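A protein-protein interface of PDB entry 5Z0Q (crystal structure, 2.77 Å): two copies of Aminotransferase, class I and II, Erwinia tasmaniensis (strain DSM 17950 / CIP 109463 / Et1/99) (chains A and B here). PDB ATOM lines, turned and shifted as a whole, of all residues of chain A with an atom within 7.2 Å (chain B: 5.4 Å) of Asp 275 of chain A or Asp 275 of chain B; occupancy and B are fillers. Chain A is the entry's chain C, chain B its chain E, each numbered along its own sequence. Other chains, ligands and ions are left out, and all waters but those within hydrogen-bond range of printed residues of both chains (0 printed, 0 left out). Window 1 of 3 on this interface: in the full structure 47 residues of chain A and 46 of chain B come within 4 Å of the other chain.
The side-chain carboxylate (OD2) of Asp 275 of chain B sits close to the backbone carbonyl oxygen (O) of Leu 247 of chain A.
O of Gly 246 of chain B sits at hydrogen-bond distance from N of Val 276 of chain A, 2.9 Å away.
The side-chain carboxylate (OD2) of Asp 275 of chain A lies close to the side-chain carboxylate (OD2) of Asp 275 of chain B (3.4 Å).
The backbone carbonyl oxygen (O) of Phe 64 of chain A lies within hydrogen-bond range of the backbone NH (N) of Gly 246 of chain B, 2.7 Å away.
The backbone carbonyl oxygen (O) of Gly 246 of chain A sits at hydrogen-bond distance from the backbone NH (N) of Val 276 of chain B (3.0 Å).
The side-chain carboxylate (OD1) of Asp 275 of chain B lies within hydrogen-bond range of the backbone NH (N) of Leu 277 of chain B, 2.6 Å away.
The backbone NH (N) of Ala 278 of chain B sits at hydrogen-bond distance from the side-chain carboxylate (OD1) of Asp 275 of chain B (3.4 Å).
OD1 of Asp 275 of chain A sits at hydrogen-bond distance from N of Leu 277 of chain A, at 2.5 Å.
Among the printed residues, merely in contact across the chains: Asp 23 of chain A with Val 276 of chain B (3.5 Å), Gly 246 of chain A with Asp 275 of chain B (3.9 Å), Leu 247 of chain A with Leu 277 of chain B (3.7 Å), Asp 275 of chain A with Gly 246 of chain B (3.6 Å), Asp 275 of chain A with Leu 247 of chain B (3.2 Å), Leu 277 of chain A with Leu 247 of chain B (3.8 Å) and Leu 277 of chain A with Leu 277 of chain B (3.6 Å).
Of chain A, only Gly 246, Leu 247 and Asp 275 come within 4 Å of Asp 275 of chain B.
Printed residues of chain B within 4 Å of Phe 64 of chain A: Gly 246 (2.7 Å).
Printed residues of chain B within 4 Å of Asp 23 of chain A: Val 276 (3.5 Å).
Ala 278 of chain A touches none of the printed residues of chain B.
The nearest residue of chain B that does not touch Asp 275 of chain A is Ala 278 of chain B (4.2 Å).
Printed residues of chain A that touch a printed residue of chain B: Asp 23, Phe 64, Gly 246, Leu 247, Asp 275, Val 276 and Leu 277.
Of the 10 printed residues of chain B, 5 touch a printed residue of chain A.
Gly 246 of chain A touches Asp 275 of chain B, and with the chains exchanged Asp 275 of chain A touches Gly 246 of chain B.
Leu 247 of chain A touches Asp 275 of chain B, and with the chains exchanged Asp 275 of chain A touches Leu 247 of chain B.
Leu 247 of chain A touches Leu 277 of chain B, and with the chains exchanged Leu 277 of chain A touches Leu 247 of chain B.
Asp 275 of chain A touches its own counterpart, Asp 275 of chain B.
Positions printed for both chains: 246, 247, 273, 274, 275, 276, 277, 278, 279 and 280.
Of the 12 pairs that touch across the chains among the printed residues, 10 have their exchanged pair printed and touching as well.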
ATOM      1  N   ASP A  23       3.765 -30.432  -4.668  1.00  0.00           N
ATOM      2  CA  ASP A  23       4.248 -29.079  -4.905  1.00  0.00           C
ATOM      3  C   ASP A  23       4.404 -28.776  -6.389  1.00  0.00           C
ATOM      4  O   ASP A  23       5.042 -27.780  -6.745  1.00  0.00           O
ATOM      5  CB  ASP A  23       5.574 -28.848  -4.174  1.00  0.00           C
ATOM      6  CG  ASP A  23       6.647 -29.844  -4.571  1.00  0.00           C
ATOM      7  OD1 ASP A  23       6.340 -30.795  -5.322  1.00  0.00           O
ATOM      8  OD2 ASP A  23       7.804 -29.676  -4.130  1.00  0.00           O
ATOM      9  N   PHE A  64      25.053 -32.692   4.345  1.00  0.00           N
ATOM     10  CA  PHE A  64      24.718 -31.896   3.167  1.00  0.00           C
ATOM     11  C   PHE A  64      25.486 -30.578   3.178  1.00  0.00           C
ATOM     12  O   PHE A  64      24.928 -29.498   2.977  1.00  0.00           O
ATOM     13  CB  PHE A  64      23.215 -31.641   3.090  1.00  0.00           C
ATOM     14  CG  PHE A  64      22.380 -32.883   3.223  1.00  0.00           C
ATOM     15  CD1 PHE A  64      22.190 -33.727   2.141  1.00  0.00           C
ATOM     16  CD2 PHE A  64      21.780 -33.203   4.431  1.00  0.00           C
ATOM     17  CE1 PHE A  64      21.419 -34.870   2.262  1.00  0.00           C
ATOM     18  CE2 PHE A  64      21.009 -34.343   4.559  1.00  0.00           C
ATOM     19  CZ  PHE A  64      20.827 -35.178   3.473  1.00  0.00           C
ATOM     20  N   VAL A  68      31.296 -30.418  -4.190  1.00  0.00           N
ATOM     21  CA  VAL A  68      32.121 -30.171  -5.357  1.00  0.00           C
ATOM     22  C   VAL A  68      31.341 -30.582  -6.597  1.00  0.00           C
ATOM     23  O   VAL A  68      30.339 -31.299  -6.527  1.00  0.00           O
ATOM     24  CB  VAL A  68      33.472 -30.917  -5.283  1.00  0.00           C
ATOM     25  CG1 VAL A  68      34.305 -30.391  -4.132  1.00  0.00           C
ATOM     26  CG2 VAL A  68      33.244 -32.417  -5.146  1.00  0.00           C
ATOM     27  N   LEU A  97      25.587 -25.743 -14.385  1.00  0.00           N
ATOM     28  CA  LEU A  97      24.673 -24.657 -14.072  1.00  0.00           C
ATOM     29  C   LEU A  97      23.430 -25.211 -13.394  1.00  0.00           C
ATOM     30  O   LEU A  97      23.075 -26.379 -13.598  1.00  0.00           O
ATOM     31  CB  LEU A  97      24.264 -23.890 -15.340  1.00  0.00           C
ATOM     32  CG  LEU A  97      25.383 -23.207 -16.126  1.00  0.00           C
ATOM     33  CD1 LEU A  97      24.942 -22.949 -17.558  1.00  0.00           C
ATOM     34  CD2 LEU A  97      25.792 -21.910 -15.447  1.00  0.00           C
ATOM     35  N   PRO A  98      22.751 -24.399 -12.573  1.00  0.00           N
ATOM     36  CA  PRO A  98      21.470 -24.818 -11.964  1.00  0.00           C
ATOM     37  C   PRO A  98      20.270 -24.465 -12.841  1.00  0.00           C
ATOM     38  O   PRO A  98      19.413 -23.638 -12.496  1.00  0.00           O
ATOM     39  CB  PRO A  98      21.477 -24.053 -10.640  1.00  0.00           C
ATOM     40  CG  PRO A  98      22.180 -22.778 -10.979  1.00  0.00           C
ATOM     41  CD  PRO A  98      23.236 -23.129 -12.004  1.00  0.00           C
ATOM     42  N   ILE A 244      13.314 -34.385 -14.217  1.00  0.00           N
ATOM     43  CA  ILE A 244      13.979 -33.934 -12.999  1.00  0.00           C
ATOM     44  C   ILE A 244      14.272 -32.441 -13.101  1.00  0.00           C
ATOM     45  O   ILE A 244      15.291 -31.958 -12.596  1.00  0.00           O
ATOM     46  CB  ILE A 244      15.267 -34.737 -12.729  1.00  0.00           C
ATOM     47  CG1 ILE A 244      16.189 -34.710 -13.949  1.00  0.00           C
ATOM     48  CG2 ILE A 244      14.931 -36.172 -12.339  1.00  0.00           C
ATOM     49  CD1 ILE A 244      17.510 -35.413 -13.724  1.00  0.00           C
ATOM     50  N   ALA A 245      13.372 -31.700 -13.753  1.00  0.00           N
ATOM     51  CA  ALA A 245      13.535 -30.256 -13.853  1.00  0.00           C
ATOM     52  C   ALA A 245      13.391 -29.564 -12.504  1.00  0.00           C
ATOM     53  O   ALA A 245      13.923 -28.462 -12.328  1.00  0.00           O
ATOM     54  CB  ALA A 245      12.526 -29.681 -14.849  1.00  0.00           C
ATOM     55  N   GLY A 246      12.693 -30.186 -11.553  1.00  0.00           N
ATOM     56  CA  GLY A 246      12.581 -29.648 -10.209  1.00  0.00           C
ATOM     57  C   GLY A 246      13.884 -29.592  -9.444  1.00  0.00           C
ATOM     58  O   GLY A 246      13.953 -28.898  -8.425  1.00  0.00           O
ATOM     59  N   LEU A 247      14.907 -30.308  -9.905  1.00  0.00           N
ATOM     60  CA  LEU A 247      16.254 -30.215  -9.358  1.00  0.00           C
ATOM     61  C   LEU A 247      17.156 -29.317 -10.193  1.00  0.00           C
ATOM     62  O   LEU A 247      17.922 -28.527  -9.636  1.00  0.00           O
ATOM     63  CB  LEU A 247      16.871 -31.612  -9.252  1.00  0.00           C
ATOM     64  CG  LEU A 247      15.965 -32.634  -8.558  1.00  0.00           C
ATOM     65  CD1 LEU A 247      16.529 -34.039  -8.657  1.00  0.00           C
ATOM     66  CD2 LEU A 247      15.741 -32.248  -7.106  1.00  0.00           C
ATOM     67  N   GLY A 248      17.082 -29.429 -11.517  1.00  0.00           N
ATOM     68  CA  GLY A 248      17.691 -28.451 -12.397  1.00  0.00           C
ATOM     69  C   GLY A 248      19.192 -28.538 -12.555  1.00  0.00           C
ATOM     70  O   GLY A 248      19.871 -27.505 -12.538  1.00  0.00           O
ATOM     71  N   ALA A 249      19.734 -29.739 -12.720  1.00  0.00           N
ATOM     72  CA  ALA A 249      21.156 -29.909 -12.985  1.00  0.00           C
ATOM     73  C   ALA A 249      21.382 -29.879 -14.492  1.00  0.00           C
ATOM     74  O   ALA A 249      20.838 -30.714 -15.223  1.00  0.00           O
ATOM     75  CB  ALA A 249      21.671 -31.214 -12.383  1.00  0.00           C
ATOM     76  N   PRO A 272      24.391 -19.410  -8.512  1.00  0.00           N
ATOM     77  CA  PRO A 272      24.980 -20.311  -7.517  1.00  0.00           C
ATOM     78  C   PRO A 272      25.406 -21.634  -8.144  1.00  0.00           C
ATOM     79  O   PRO A 272      25.217 -21.883  -9.334  1.00  0.00           O
ATOM     80  CB  PRO A 272      23.838 -20.509  -6.517  1.00  0.00           C
ATOM     81  CG  PRO A 272      22.606 -20.369  -7.346  1.00  0.00           C
ATOM     82  CD  PRO A 272      22.926 -19.321  -8.382  1.00  0.00           C
ATOM     83  N   ASP A 273      25.994 -22.489  -7.310  1.00  0.00           N
ATOM     84  CA  ASP A 273      26.406 -23.815  -7.738  1.00  0.00           C
ATOM     85  C   ASP A 273      25.213 -24.768  -7.750  1.00  0.00           C
ATOM     86  O   ASP A 273      24.138 -24.476  -7.218  1.00  0.00           O
ATOM     87  CB  ASP A 273      27.509 -24.356  -6.828  1.00  0.00           C
ATOM     88  CG  ASP A 273      28.825 -23.625  -7.007  1.00  0.00           C
ATOM     89  OD1 ASP A 273      29.030 -23.023  -8.082  1.00  0.00           O
ATOM     90  OD2 ASP A 273      29.657 -23.658  -6.075  1.00  0.00           O
ATOM     91  N   VAL A 274      25.418 -25.931  -8.371  1.00  0.00           N
ATOM     92  CA  VAL A 274      24.352 -26.916  -8.485  1.00  0.00           C
ATOM     93  C   VAL A 274      24.105 -27.573  -7.131  1.00  0.00           C
ATOM     94  O   VAL A 274      25.026 -27.760  -6.324  1.00  0.00           O
ATOM     95  CB  VAL A 274      24.705 -27.961  -9.560  1.00  0.00           C
ATOM     96  CG1 VAL A 274      23.561 -28.947  -9.761  1.00  0.00           C
ATOM     97  CG2 VAL A 274      25.052 -27.271 -10.872  1.00  0.00           C
ATOM     98  N   ASP A 275      22.842 -27.909  -6.874  1.00  0.00           N
ATOM     99  CA  ASP A 275      22.468 -28.604  -5.651  1.00  0.00           C
ATOM    100  C   ASP A 275      23.251 -29.907  -5.514  1.00  0.00           C
ATOM    101  O   ASP A 275      23.571 -30.577  -6.501  1.00  0.00           O
ATOM    102  CB  ASP A 275      20.961 -28.884  -5.653  1.00  0.00           C
ATOM    103  CG  ASP A 275      20.454 -29.433  -4.329  1.00  0.00           C
ATOM    104  OD1 ASP A 275      20.962 -30.478  -3.867  1.00  0.00           O
ATOM    105  OD2 ASP A 275      19.537 -28.816  -3.746  1.00  0.00           O
ATOM    106  N   VAL A 276      23.566 -30.259  -4.264  1.00  0.00           N
ATOM    107  CA  VAL A 276      24.282 -31.503  -3.993  1.00  0.00           C
ATOM    108  C   VAL A 276      23.459 -32.702  -4.446  1.00  0.00           C
ATOM    109  O   VAL A 276      23.990 -33.654  -5.036  1.00  0.00           O
ATOM    110  CB  VAL A 276      24.645 -31.588  -2.499  1.00  0.00           C
ATOM    111  CG1 VAL A 276      24.761 -33.034  -2.052  1.00  0.00           C
ATOM    112  CG2 VAL A 276      25.944 -30.845  -2.228  1.00  0.00           C
ATOM    113  N   LEU A 277      22.149 -32.672  -4.193  1.00  0.00           N
ATOM    114  CA  LEU A 277      21.281 -33.770  -4.603  1.00  0.00           C
ATOM    115  C   LEU A 277      21.001 -33.753  -6.099  1.00  0.00           C
ATOM    116  O   LEU A 277      20.738 -34.808  -6.686  1.00  0.00           O
ATOM    117  CB  LEU A 277      19.968 -33.717  -3.820  1.00  0.00           C
ATOM    118  CG  LEU A 277      20.100 -33.851  -2.301  1.00  0.00           C
ATOM    119  CD1 LEU A 277      18.773 -33.589  -1.616  1.00  0.00           C
ATOM    120  CD2 LEU A 277      20.622 -35.227  -1.934  1.00  0.00           C
ATOM    121  N   ALA A 278      21.051 -32.579  -6.733  1.00  0.00           N
ATOM    122  CA  ALA A 278      20.808 -32.506  -8.169  1.00  0.00           C
ATOM    123  C   ALA A 278      21.920 -33.179  -8.962  1.00  0.00           C
ATOM    124  O   ALA A 278      21.659 -33.768 -10.017  1.00  0.00           O
ATOM    125  CB  ALA A 278      20.650 -31.049  -8.602  1.00  0.00           C
ATOM    126  N   TYR A 279      23.162 -33.098  -8.478  1.00  0.00           N
ATOM    127  CA  TYR A 279      24.258 -33.801  -9.133  1.00  0.00           C
ATOM    128  C   TYR A 279      24.041 -35.308  -9.105  1.00  0.00           C
ATOM    129  O   TYR A 279      24.330 -36.004 -10.085  1.00  0.00           O
ATOM    130  CB  TYR A 279      25.585 -33.445  -8.464  1.00  0.00           C
ATOM    131  CG  TYR A 279      26.256 -32.208  -9.016  1.00  0.00           C
ATOM    132  CD1 TYR A 279      26.248 -31.938 -10.378  1.00  0.00           C
ATOM    133  CD2 TYR A 279      26.902 -31.313  -8.174  1.00  0.00           C
ATOM    134  CE1 TYR A 279      26.864 -30.808 -10.885  1.00  0.00           C
ATOM    135  CE2 TYR A 279      27.519 -30.182  -8.671  1.00  0.00           C
ATOM    136  CZ  TYR A 279      27.499 -29.936 -10.025  1.00  0.00           C
ATOM    137  OH  TYR A 279      28.114 -28.809 -10.519  1.00  0.00           O
ATOM    138  N   VAL A 280      23.530 -35.828  -7.986  1.00  0.00           N
ATOM    139  CA  VAL A 280      23.350 -37.270  -7.845  1.00  0.00           C
ATOM    140  C   VAL A 280      22.274 -37.772  -8.798  1.00  0.00           C
ATOM    141  O   VAL A 280      22.411 -38.842  -9.405  1.00  0.00           O
ATOM    142  CB  VAL A 280      23.027 -37.619  -6.381  1.00  0.00           C
ATOM    143  CG1 VAL A 280      22.722 -39.098  -6.238  1.00  0.00           C
ATOM    144  CG2 VAL A 280      24.184 -37.226  -5.475  1.00  0.00           C
ATOM    145  N   GLY B 246      24.678 -27.424   1.197  1.00  0.00           N
ATOM    146  CA  GLY B 246      24.673 -28.141  -0.065  1.00  0.00           C
ATOM    147  C   GLY B 246      23.362 -28.066  -0.817  1.00  0.00           C
ATOM    148  O   GLY B 246      23.312 -28.470  -1.984  1.00  0.00           O
ATOM    149  N   LEU B 247      22.307 -27.572  -0.174  1.00  0.00           N
ATOM    150  CA  LEU B 247      21.014 -27.341  -0.806  1.00  0.00           C
ATOM    151  C   LEU B 247      20.692 -25.865  -0.955  1.00  0.00           C
ATOM    152  O   LEU B 247      20.084 -25.467  -1.951  1.00  0.00           O
ATOM    153  CB  LEU B 247      19.910 -28.029   0.003  1.00  0.00           C
ATOM    154  CG  LEU B 247      20.289 -29.425   0.505  1.00  0.00           C
ATOM    155  CD1 LEU B 247      19.251 -29.958   1.474  1.00  0.00           C
ATOM    156  CD2 LEU B 247      20.480 -30.389  -0.656  1.00  0.00           C
ATOM    157  N   ASP B 273      14.936 -20.700  -9.628  1.00  0.00           N
ATOM    158  CA  ASP B 273      14.123 -20.960  -8.452  1.00  0.00           C
ATOM    159  C   ASP B 273      14.867 -21.870  -7.479  1.00  0.00           C
ATOM    160  O   ASP B 273      15.864 -22.512  -7.822  1.00  0.00           O
ATOM    161  CB  ASP B 273      12.793 -21.600  -8.852  1.00  0.00           C
ATOM    162  CG  ASP B 273      11.962 -20.708  -9.755  1.00  0.00           C
ATOM    163  OD1 ASP B 273      11.788 -19.517  -9.420  1.00  0.00           O
ATOM    164  OD2 ASP B 273      11.487 -21.198 -10.803  1.00  0.00           O
ATOM    165  N   VAL B 274      14.367 -21.920  -6.244  1.00  0.00           N
ATOM    166  CA  VAL B 274      14.953 -22.796  -5.238  1.00  0.00           C
ATOM    167  C   VAL B 274      14.633 -24.244  -5.581  1.00  0.00           C
ATOM    168  O   VAL B 274      13.530 -24.564  -6.050  1.00  0.00           O
ATOM    169  CB  VAL B 274      14.445 -22.418  -3.835  1.00  0.00           C
ATOM    170  CG1 VAL B 274      14.970 -23.388  -2.785  1.00  0.00           C
ATOM    171  CG2 VAL B 274      14.860 -20.998  -3.489  1.00  0.00           C
ATOM    172  N   ASP B 275      15.608 -25.127  -5.361  1.00  0.00           N
ATOM    173  CA  ASP B 275      15.446 -26.547  -5.647  1.00  0.00           C
ATOM    174  C   ASP B 275      14.231 -27.112  -4.915  1.00  0.00           C
ATOM    175  O   ASP B 275      13.873 -26.668  -3.820  1.00  0.00           O
ATOM    176  CB  ASP B 275      16.721 -27.298  -5.244  1.00  0.00           C
ATOM    177  CG  ASP B 275      16.687 -28.770  -5.618  1.00  0.00           C
ATOM    178  OD1 ASP B 275      15.870 -29.522  -5.046  1.00  0.00           O
ATOM    179  OD2 ASP B 275      17.487 -29.176  -6.489  1.00  0.00           O
ATOM    180  N   VAL B 276      13.592 -28.104  -5.541  1.00  0.00           N
ATOM    181  CA  VAL B 276      12.407 -28.726  -4.952  1.00  0.00           C
ATOM    182  C   VAL B 276      12.757 -29.389  -3.624  1.00  0.00           C
ATOM    183  O   VAL B 276      12.042 -29.237  -2.625  1.00  0.00           O
ATOM    184  CB  VAL B 276      11.782 -29.728  -5.939  1.00  0.00           C
ATOM    185  CG1 VAL B 276      10.938 -30.752  -5.204  1.00  0.00           C
ATOM    186  CG2 VAL B 276      10.939 -28.995  -6.970  1.00  0.00           C
ATOM    187  N   LEU B 277      13.865 -30.132  -3.591  1.00  0.00           N
ATOM    188  CA  LEU B 277      14.283 -30.778  -2.351  1.00  0.00           C
ATOM    189  C   LEU B 277      14.816 -29.769  -1.340  1.00  0.00           C
ATOM    190  O   LEU B 277      14.717 -29.997  -0.128  1.00  0.00           O
ATOM    191  CB  LEU B 277      15.335 -31.847  -2.647  1.00  0.00           C
ATOM    192  CG  LEU B 277      14.825 -33.069  -3.413  1.00  0.00           C
ATOM    193  CD1 LEU B 277      15.975 -33.963  -3.836  1.00  0.00           C
ATOM    194  CD2 LEU B 277      13.832 -33.847  -2.568  1.00  0.00           C
ATOM    195  N   ALA B 278      15.376 -28.652  -1.813  1.00  0.00           N
ATOM    196  CA  ALA B 278      15.884 -27.635  -0.897  1.00  0.00           C
ATOM    197  C   ALA B 278      14.755 -26.994  -0.100  1.00  0.00           C
ATOM    198  O   ALA B 278      14.924 -26.681   1.085  1.00  0.00           O
ATOM    199  CB  ALA B 278      16.669 -26.577  -1.670  1.00  0.00           C
ATOM    200  N   TYR B 279      13.596 -26.790  -0.735  1.00  0.00           N
ATOM    201  CA  TYR B 279      12.441 -26.253  -0.020  1.00  0.00           C
ATOM    202  C   TYR B 279      12.027 -27.168   1.126  1.00  0.00           C
ATOM    203  O   TYR B 279      11.753 -26.699   2.236  1.00  0.00           O
ATOM    204  CB  TYR B 279      11.274 -26.056  -0.986  1.00  0.00           C
ATOM    205  CG  TYR B 279      11.199 -24.684  -1.619  1.00  0.00           C
ATOM    206  CD1 TYR B 279      11.402 -23.535  -0.866  1.00  0.00           C
ATOM    207  CD2 TYR B 279      10.918 -24.540  -2.972  1.00  0.00           C
ATOM    208  CE1 TYR B 279      11.329 -22.280  -1.443  1.00  0.00           C
ATOM    209  CE2 TYR B 279      10.844 -23.292  -3.559  1.00  0.00           C
ATOM    210  CZ  TYR B 279      11.049 -22.166  -2.791  1.00  0.00           C
ATOM    211  OH  TYR B 279      10.974 -20.923  -3.377  1.00  0.00           O
ATOM    212  N   VAL B 280      11.980 -28.477   0.873  1.00  0.00           N
ATOM    213  CA  VAL B 280      11.528 -29.425   1.887  1.00  0.00           C
ATOM    214  C   VAL B 280      12.496 -29.464   3.063  1.00  0.00           C
ATOM    215  O   VAL B 280      12.079 -29.448   4.228  1.00  0.00           O
ATOM    216  CB  VAL B 280      11.341 -30.818   1.259  1.00  0.00           C
ATOM    217  CG1 VAL B 280      11.232 -31.878   2.340  1.00  0.00           C
ATOM    218  CG2 VAL B 280      10.107 -30.833   0.366  1.00  0.00           C
